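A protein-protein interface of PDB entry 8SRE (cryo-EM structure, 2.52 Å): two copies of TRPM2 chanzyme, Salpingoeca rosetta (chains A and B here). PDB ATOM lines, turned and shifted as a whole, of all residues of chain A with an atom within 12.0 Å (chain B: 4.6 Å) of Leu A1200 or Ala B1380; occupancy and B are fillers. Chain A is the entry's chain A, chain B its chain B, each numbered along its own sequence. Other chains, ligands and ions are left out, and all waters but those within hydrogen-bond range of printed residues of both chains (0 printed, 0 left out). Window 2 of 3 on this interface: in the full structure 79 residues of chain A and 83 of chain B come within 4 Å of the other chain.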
ATOM      1  N   PRO A1196      28.829 -16.629 -21.671  1.00  0.00           N
ATOM      2  CA  PRO A1196      27.375 -16.591 -21.482  1.00  0.00           C
ATOM      3  C   PRO A1196      26.974 -15.880 -20.193  1.00  0.00           C
ATOM      4  O   PRO A1196      26.148 -14.967 -20.228  1.00  0.00           O
ATOM      5  CB  PRO A1196      26.991 -18.072 -21.432  1.00  0.00           C
ATOM      6  N   ILE A1197      27.559 -16.295 -19.074  1.00  0.00           N
ATOM      7  CA  ILE A1197      27.290 -15.683 -17.779  1.00  0.00           C
ATOM      8  C   ILE A1197      28.094 -14.394 -17.698  1.00  0.00           C
ATOM      9  O   ILE A1197      29.296 -14.400 -17.995  1.00  0.00           O
ATOM     10  CB  ILE A1197      27.648 -16.631 -16.625  1.00  0.00           C
ATOM     11  N   ASN A1198      27.418 -13.311 -17.270  1.00  0.00           N
ATOM     12  CA  ASN A1198      27.840 -11.901 -17.294  1.00  0.00           C
ATOM     13  C   ASN A1198      28.330 -11.451 -18.670  1.00  0.00           C
ATOM     14  O   ASN A1198      29.500 -11.088 -18.833  1.00  0.00           O
ATOM     15  CB  ASN A1198      28.891 -11.587 -16.219  1.00  0.00           C
ATOM     16  N   ARG A1199      27.439 -11.465 -19.659  1.00  0.00           N
ATOM     17  CA  ARG A1199      27.735 -11.074 -21.034  1.00  0.00           C
ATOM     18  C   ARG A1199      26.512 -10.361 -21.582  1.00  0.00           C
ATOM     19  O   ARG A1199      25.400 -10.894 -21.555  1.00  0.00           O
ATOM     20  CB  ARG A1199      28.058 -12.260 -21.962  1.00  0.00           C
ATOM     21  CG  ARG A1199      29.266 -13.159 -21.663  1.00  0.00           C
ATOM     22  CD  ARG A1199      30.562 -12.389 -21.824  1.00  0.00           C
ATOM     23  NE  ARG A1199      30.784 -11.969 -23.198  1.00  0.00           N
ATOM     24  CZ  ARG A1199      31.874 -11.345 -23.622  1.00  0.00           C
ATOM     25  NH1 ARG A1199      32.853 -11.027 -22.792  1.00  0.00           N
ATOM     26  NH2 ARG A1199      31.974 -11.014 -24.906  1.00  0.00           N
ATOM     27  N   LEU A1200      26.720  -9.151 -22.086  1.00  0.00           N
ATOM     28  CA  LEU A1200      25.614  -8.308 -22.502  1.00  0.00           C
ATOM     29  C   LEU A1200      25.911  -7.754 -23.891  1.00  0.00           C
ATOM     30  O   LEU A1200      27.039  -7.349 -24.180  1.00  0.00           O
ATOM     31  CB  LEU A1200      25.389  -7.191 -21.476  1.00  0.00           C
ATOM     32  CG  LEU A1200      24.182  -6.285 -21.660  1.00  0.00           C
ATOM     33  CD1 LEU A1200      22.960  -7.170 -21.521  1.00  0.00           C
ATOM     34  CD2 LEU A1200      24.144  -5.211 -20.636  1.00  0.00           C
ATOM     35  N   ASN A1201      24.886  -7.729 -24.740  1.00  0.00           N
ATOM     36  CA  ASN A1201      24.976  -7.248 -26.113  1.00  0.00           C
ATOM     37  C   ASN A1201      24.167  -5.970 -26.281  1.00  0.00           C
ATOM     38  O   ASN A1201      22.935  -5.994 -26.211  1.00  0.00           O
ATOM     39  CB  ASN A1201      24.462  -8.326 -27.069  1.00  0.00           C
ATOM     40  CG  ASN A1201      24.886  -8.098 -28.500  1.00  0.00           C
ATOM     41  OD1 ASN A1201      25.933  -7.529 -28.762  1.00  0.00           O
ATOM     42  ND2 ASN A1201      24.066  -8.554 -29.438  1.00  0.00           N
ATOM     43  N   SER A1202      24.873  -4.861 -26.517  1.00  0.00           N
ATOM     44  CA  SER A1202      24.291  -3.532 -26.667  1.00  0.00           C
ATOM     45  C   SER A1202      24.314  -3.038 -28.106  1.00  0.00           C
ATOM     46  O   SER A1202      24.232  -1.828 -28.337  1.00  0.00           O
ATOM     47  CB  SER A1202      24.986  -2.520 -25.767  1.00  0.00           C
ATOM     48  OG  SER A1202      24.660  -2.746 -24.410  1.00  0.00           O
ATOM     49  N   ALA A1203      24.466  -3.950 -29.077  1.00  0.00           N
ATOM     50  CA  ALA A1203      24.466  -3.613 -30.503  1.00  0.00           C
ATOM     51  C   ALA A1203      23.103  -3.147 -31.022  1.00  0.00           C
ATOM     52  O   ALA A1203      23.055  -2.521 -32.090  1.00  0.00           O
ATOM     53  CB  ALA A1203      24.940  -4.813 -31.320  1.00  0.00           C
ATOM     54  N   VAL A1204      22.006  -3.506 -30.328  1.00  0.00           N
ATOM     55  CA  VAL A1204      20.627  -3.117 -30.643  1.00  0.00           C
ATOM     56  C   VAL A1204      20.431  -1.592 -30.561  1.00  0.00           C
ATOM     57  O   VAL A1204      19.617  -1.025 -31.303  1.00  0.00           O
ATOM     58  CB  VAL A1204      19.682  -3.893 -29.685  1.00  0.00           C
ATOM     59  CG1 VAL A1204      18.198  -3.815 -30.082  1.00  0.00           C
ATOM     60  CG2 VAL A1204      20.105  -5.357 -29.564  1.00  0.00           C
ATOM     61  N   ALA A1205      21.188  -0.903 -29.679  1.00  0.00           N
ATOM     62  CA  ALA A1205      21.168   0.560 -29.571  1.00  0.00           C
ATOM     63  C   ALA A1205      21.748   1.265 -30.799  1.00  0.00           C
ATOM     64  O   ALA A1205      21.386   2.411 -31.081  1.00  0.00           O
ATOM     65  CB  ALA A1205      21.926   0.997 -28.320  1.00  0.00           C
ATOM     66  N   VAL A1206      22.635   0.597 -31.534  1.00  0.00           N
ATOM     67  CA  VAL A1206      23.336   1.169 -32.672  1.00  0.00           C
ATOM     68  C   VAL A1206      22.522   0.802 -33.908  1.00  0.00           C
ATOM     69  O   VAL A1206      22.133   1.671 -34.696  1.00  0.00           O
ATOM     70  CB  VAL A1206      24.792   0.669 -32.747  1.00  0.00           C
ATOM     71  CG1 VAL A1206      25.419   0.884 -34.135  1.00  0.00           C
ATOM     72  CG2 VAL A1206      25.612   1.295 -31.655  1.00  0.00           C
ATOM     73  N   HIS A1207      22.257  -0.501 -34.077  1.00  0.00           N
ATOM     74  CA  HIS A1207      21.595  -1.004 -35.274  1.00  0.00           C
ATOM     75  C   HIS A1207      20.079  -0.851 -35.243  1.00  0.00           C
ATOM     76  O   HIS A1207      19.524  -0.182 -36.119  1.00  0.00           O
ATOM     77  CB  HIS A1207      21.959  -2.473 -35.472  1.00  0.00           C
ATOM     78  CG  HIS A1207      23.347  -2.685 -35.986  1.00  0.00           C
ATOM     79  ND1 HIS A1207      23.709  -2.422 -37.289  1.00  0.00           N
ATOM     80  CD2 HIS A1207      24.464  -3.139 -35.370  1.00  0.00           C
ATOM     81  CE1 HIS A1207      24.990  -2.702 -37.453  1.00  0.00           C
ATOM     82  NE2 HIS A1207      25.472  -3.140 -36.303  1.00  0.00           N
ATOM     83  N   GLY A1208      19.399  -1.443 -34.264  1.00  0.00           N
ATOM     84  CA  GLY A1208      17.950  -1.347 -34.208  1.00  0.00           C
ATOM     85  C   GLY A1208      17.252  -2.673 -34.473  1.00  0.00           C
ATOM     86  O   GLY A1208      17.396  -3.640 -33.724  1.00  0.00           O
ATOM     87  N   ALA A1211      19.618  -7.294 -37.076  1.00  0.00           N
ATOM     88  CA  ALA A1211      20.413  -8.226 -36.285  1.00  0.00           C
ATOM     89  C   ALA A1211      20.667  -9.468 -37.130  1.00  0.00           C
ATOM     90  O   ALA A1211      20.505  -9.445 -38.356  1.00  0.00           O
ATOM     91  CB  ALA A1211      19.711  -8.567 -34.966  1.00  0.00           C
ATOM     92  N   ASP B1378      15.279  -2.963 -21.799  1.00  0.00           N
ATOM     93  CA  ASP B1378      16.216  -3.679 -20.954  1.00  0.00           C
ATOM     94  C   ASP B1378      17.462  -2.826 -20.737  1.00  0.00           C
ATOM     95  O   ASP B1378      17.540  -1.696 -21.216  1.00  0.00           O
ATOM     96  CB  ASP B1378      16.528  -5.064 -21.544  1.00  0.00           C
ATOM     97  CG  ASP B1378      17.068  -5.026 -22.985  1.00  0.00           C
ATOM     98  OD1 ASP B1378      17.048  -3.977 -23.666  1.00  0.00           O
ATOM     99  OD2 ASP B1378      17.520  -6.092 -23.448  1.00  0.00           O
ATOM    100  N   VAL B1379      18.414  -3.368 -19.964  1.00  0.00           N
ATOM    101  CA  VAL B1379      19.662  -2.680 -19.616  1.00  0.00           C
ATOM    102  C   VAL B1379      20.579  -2.517 -20.838  1.00  0.00           C
ATOM    103  O   VAL B1379      21.316  -1.515 -20.939  1.00  0.00           O
ATOM    104  CB  VAL B1379      20.312  -3.478 -18.455  1.00  0.00           C
ATOM    105  CG1 VAL B1379      21.579  -2.849 -17.884  1.00  0.00           C
ATOM    106  CG2 VAL B1379      19.301  -3.696 -17.343  1.00  0.00           C
ATOM    107  N   ALA B1380      20.497  -3.483 -21.783  1.00  0.00           N
ATOM    108  CA  ALA B1380      21.266  -3.558 -23.038  1.00  0.00           C
ATOM    109  C   ALA B1380      21.062  -2.347 -23.944  1.00  0.00           C
ATOM    110  O   ALA B1380      22.032  -1.761 -24.438  1.00  0.00           O
ATOM    111  CB  ALA B1380      20.886  -4.828 -23.792  1.00  0.00           C
ATOM    112  N   LEU B1381      19.798  -2.023 -24.233  1.00  0.00           N
ATOM    113  CA  LEU B1381      19.455  -0.853 -25.034  1.00  0.00           C
ATOM    114  C   LEU B1381      19.762   0.448 -24.290  1.00  0.00           C
ATOM    115  O   LEU B1381      20.239   1.408 -24.911  1.00  0.00           O
ATOM    116  CB  LEU B1381      17.991  -0.941 -25.467  1.00  0.00           C
ATOM    117  CG  LEU B1381      17.304   0.180 -26.243  1.00  0.00           C
ATOM    118  CD1 LEU B1381      18.055   0.531 -27.488  1.00  0.00           C
ATOM    119  CD2 LEU B1381      15.944  -0.319 -26.655  1.00  0.00           C
ATOM    120  N   THR B1382      19.456   0.478 -22.973  1.00  0.00           N
ATOM    121  CA  THR B1382      19.520   1.680 -22.127  1.00  0.00           C
ATOM    122  C   THR B1382      20.942   2.204 -21.948  1.00  0.00           C
ATOM    123  O   THR B1382      21.163   3.418 -22.093  1.00  0.00           O
ATOM    124  CB  THR B1382      18.902   1.376 -20.762  1.00  0.00           C
ATOM    125  OG1 THR B1382      17.609   0.795 -20.953  1.00  0.00           O
ATOM    126  CG2 THR B1382      18.747   2.618 -19.919  1.00  0.00           C
ATOM    127  N   SER B1383      21.898   1.281 -21.674  1.00  0.00           N
ATOM    128  CA  SER B1383      23.326   1.558 -21.434  1.00  0.00           C
ATOM    129  C   SER B1383      23.971   2.198 -22.653  1.00  0.00           C
ATOM    130  O   SER B1383      24.641   3.247 -22.548  1.00  0.00           O
ATOM    131  CB  SER B1383      24.053   0.270 -21.058  1.00  0.00           C
ATOM    132  OG  SER B1383      23.665  -0.789 -21.911  1.00  0.00           O
ATOM    133  N   GLY B1384      23.741   1.552 -23.810  1.00  0.00           N
ATOM    134  CA  GLY B1384      24.221   2.020 -25.095  1.00  0.00           C
ATOM    135  C   GLY B1384      23.616   3.352 -25.504  1.00  0.00           C
ATOM    136  O   GLY B1384      24.357   4.245 -25.917  1.00  0.00           O
ATOM    137  N   PHE B1413      30.459  -2.275 -28.636  1.00  0.00           N
ATOM    138  CA  PHE B1413      29.284  -2.543 -27.813  1.00  0.00           C
ATOM    139  C   PHE B1413      28.858  -4.002 -27.840  1.00  0.00           C
ATOM    140  O   PHE B1413      27.928  -4.368 -27.116  1.00  0.00           O
ATOM    141  CB  PHE B1413      28.109  -1.680 -28.297  1.00  0.00           C
ATOM    142  CG  PHE B1413      28.073  -0.251 -27.766  1.00  0.00           C
ATOM    143  CD1 PHE B1413      29.165   0.352 -27.096  1.00  0.00           C
ATOM    144  CD2 PHE B1413      26.939   0.526 -28.048  1.00  0.00           C
ATOM    145  CE1 PHE B1413      29.092   1.677 -26.660  1.00  0.00           C
ATOM    146  CE2 PHE B1413      26.859   1.857 -27.632  1.00  0.00           C
ATOM    147  CZ  PHE B1413      27.934   2.421 -26.932  1.00  0.00           C
ATOM    148  N   SER B1414      29.507  -4.842 -28.649  1.00  0.00           N
ATOM    149  CA  SER B1414      29.098  -6.239 -28.728  1.00  0.00           C
ATOM    150  C   SER B1414      29.672  -7.088 -27.599  1.00  0.00           C
ATOM    151  O   SER B1414      29.209  -8.213 -27.376  1.00  0.00           O
ATOM    152  CB  SER B1414      29.505  -6.821 -30.078  1.00  0.00           C
ATOM    153  OG  SER B1414      30.888  -6.630 -30.307  1.00  0.00           O
ATOM    154  N   SER B1415      30.664  -6.587 -26.876  1.00  0.00           N
ATOM    155  CA  SER B1415      31.295  -7.353 -25.801  1.00  0.00           C
ATOM    156  C   SER B1415      31.249  -6.554 -24.507  1.00  0.00           C
ATOM    157  O   SER B1415      32.184  -5.817 -24.189  1.00  0.00           O
ATOM    158  CB  SER B1415      32.729  -7.716 -26.171  1.00  0.00           C
ATOM    159  OG  SER B1415      33.461  -6.567 -26.557  1.00  0.00           O
ATOM    160  N   GLY B1416      30.169  -6.702 -23.755  1.00  0.00           N
ATOM    161  CA  GLY B1416      30.041  -6.017 -22.486  1.00  0.00           C
ATOM    162  C   GLY B1416      29.784  -6.988 -21.360  1.00  0.00           C
ATOM    163  O   GLY B1416      29.057  -7.968 -21.511  1.00  0.00           O
ATOM    164  N   ILE B1418      28.614  -7.265 -17.279  1.00  0.00           N
ATOM    165  CA  ILE B1418      27.961  -6.654 -16.128  1.00  0.00           C
ATOM    166  C   ILE B1418      28.889  -6.876 -14.937  1.00  0.00           C
ATOM    167  O   ILE B1418      29.106  -8.010 -14.501  1.00  0.00           O
ATOM    168  CB  ILE B1418      26.565  -7.227 -15.897  1.00  0.00           C
ATOM    169  CG1 ILE B1418      25.649  -6.812 -17.050  1.00  0.00           C
ATOM    170  CG2 ILE B1418      25.988  -6.713 -14.577  1.00  0.00           C
ATOM    171  CD1 ILE B1418      24.231  -7.347 -16.970  1.00  0.00           C
ATOM    172  N   VAL B1440      27.558  -1.645 -16.625  1.00  0.00           N
ATOM    173  CA  VAL B1440      28.024  -2.384 -17.794  1.00  0.00           C
ATOM    174  C   VAL B1440      29.358  -1.813 -18.244  1.00  0.00           C
ATOM    175  O   VAL B1440      29.470  -0.609 -18.498  1.00  0.00           O
ATOM    176  CB  VAL B1440      27.021  -2.306 -18.961  1.00  0.00           C
ATOM    177  CG1 VAL B1440      27.371  -3.330 -20.005  1.00  0.00           C
ATOM    178  CG2 VAL B1440      25.574  -2.442 -18.510  1.00  0.00           C
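O of Ala B1380 sits at hydrogen-bond distance from OG of Ser B1383 (3.2 Å). OG of Ser B1383 sits at hydrogen-bond distance from O of Val B1379. The backbone NH (N) of Leu B1381 is in hydrogen-bond range of the side-chain carboxylate (OD1) of Asp B1378 (3.4 Å).
No position is printed for both chains.
Of the printed residues of chain B, Leu A1200 touches Ala B1380 (3.9 Å), Ser B1414 (3.96 Å), Gly B1416 (2.7 Å) and Val B1440 (3.8 Å). Ala B1380 touches just these residues of chain A: Leu A1200 (3.9 Å), Asn A1201 (3.4 Å) and Ser A1202 (2.8 Å). Leu B1381 touches one residue of chain A. No residue of chain A comes within 4 Å of Thr B1382. Ser B1383 touches one residue of chain A. Ser B1414 touches two residues of chain A. Of the printed residues of chain A, Ser B1415 touches Arg A1199. Ile B1418 touches one residue of chain A. Printed residues of chain A within 4 Å of Val B1440: Leu A1200 (3.8 Å). Of the printed residues of chain B, Arg A1199 touches Ser B1415 (3.6 Å) and Gly B1416 (3.4 Å). Of the printed residues of chain B, Ser A1202 touches Ala B1380 (2.8 Å), Ser B1383 (3.3 Å) and Phe B1413 (3.2 Å). Of the printed residues of chain B, Val A1206 touches Phe B1413 (3.9 Å). Of the printed residues of chain B, Asn A1201 touches Ala B1380 (3.4 Å) and Ser B1414 (3.4 Å). Pro A1196 touches none of the printed residues of chain B. The nearest residue of chain B that does not touch Leu A1200 is Ile B1418 (4.2 Å).
N of Ser A1202 lies within hydrogen-bond range of O of Phe B1413 (3.2 Å). The side-chain hydroxyl (OG) of Ser A1202 lies within hydrogen-bond range of the backbone carbonyl oxygen (O) of Ala B1380 (2.8 Å). The backbone carbonyl oxygen of Gly B1416 sits at hydrogen-bond distance from the backbone NH of Leu A1200 (2.7 Å). The side-chain hydroxyl (OG) of Ser B1383 lies within hydrogen-bond range of the side-chain hydroxyl (OG) of Ser A1202.
Hydrophobic or aromatic side chains of chain A that line the printed part of chain B: Leu A1200, Ala A1205 and Val A1206. Of the 13 printed residues of chain B, 9 touch a printed residue of chain A. Among the printed residues, no Asp or Glu carboxylate lies within 4 Å of a Lys or Arg side-chain nitrogen of the other chain.
Asn A1198 touches Ile B1418. Arg A1199 touches Ser B1415 (NH2 to CB, 3.6 Å). CA of Arg A1199 touches O of Gly B1416 (3.4 Å). Leu A1200 touches Ala B1380. Leu A1200 touches Ser B1414 (O to O, 3.96 Å). CG2 of Val B1440 touches CD2 of Leu A1200, 3.8 Å away. O of Asn A1201 touches CB of Ala B1380, 3.4 Å away. Asn A1201 touches Ser B1414 (OD1 to CA, 3.4 Å). CA of Ala A1205 touches CD1 of Leu B1381 (3.7 Å). CD2 of Phe B1413 touches CG2 of Val A1206 (3.9 Å).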
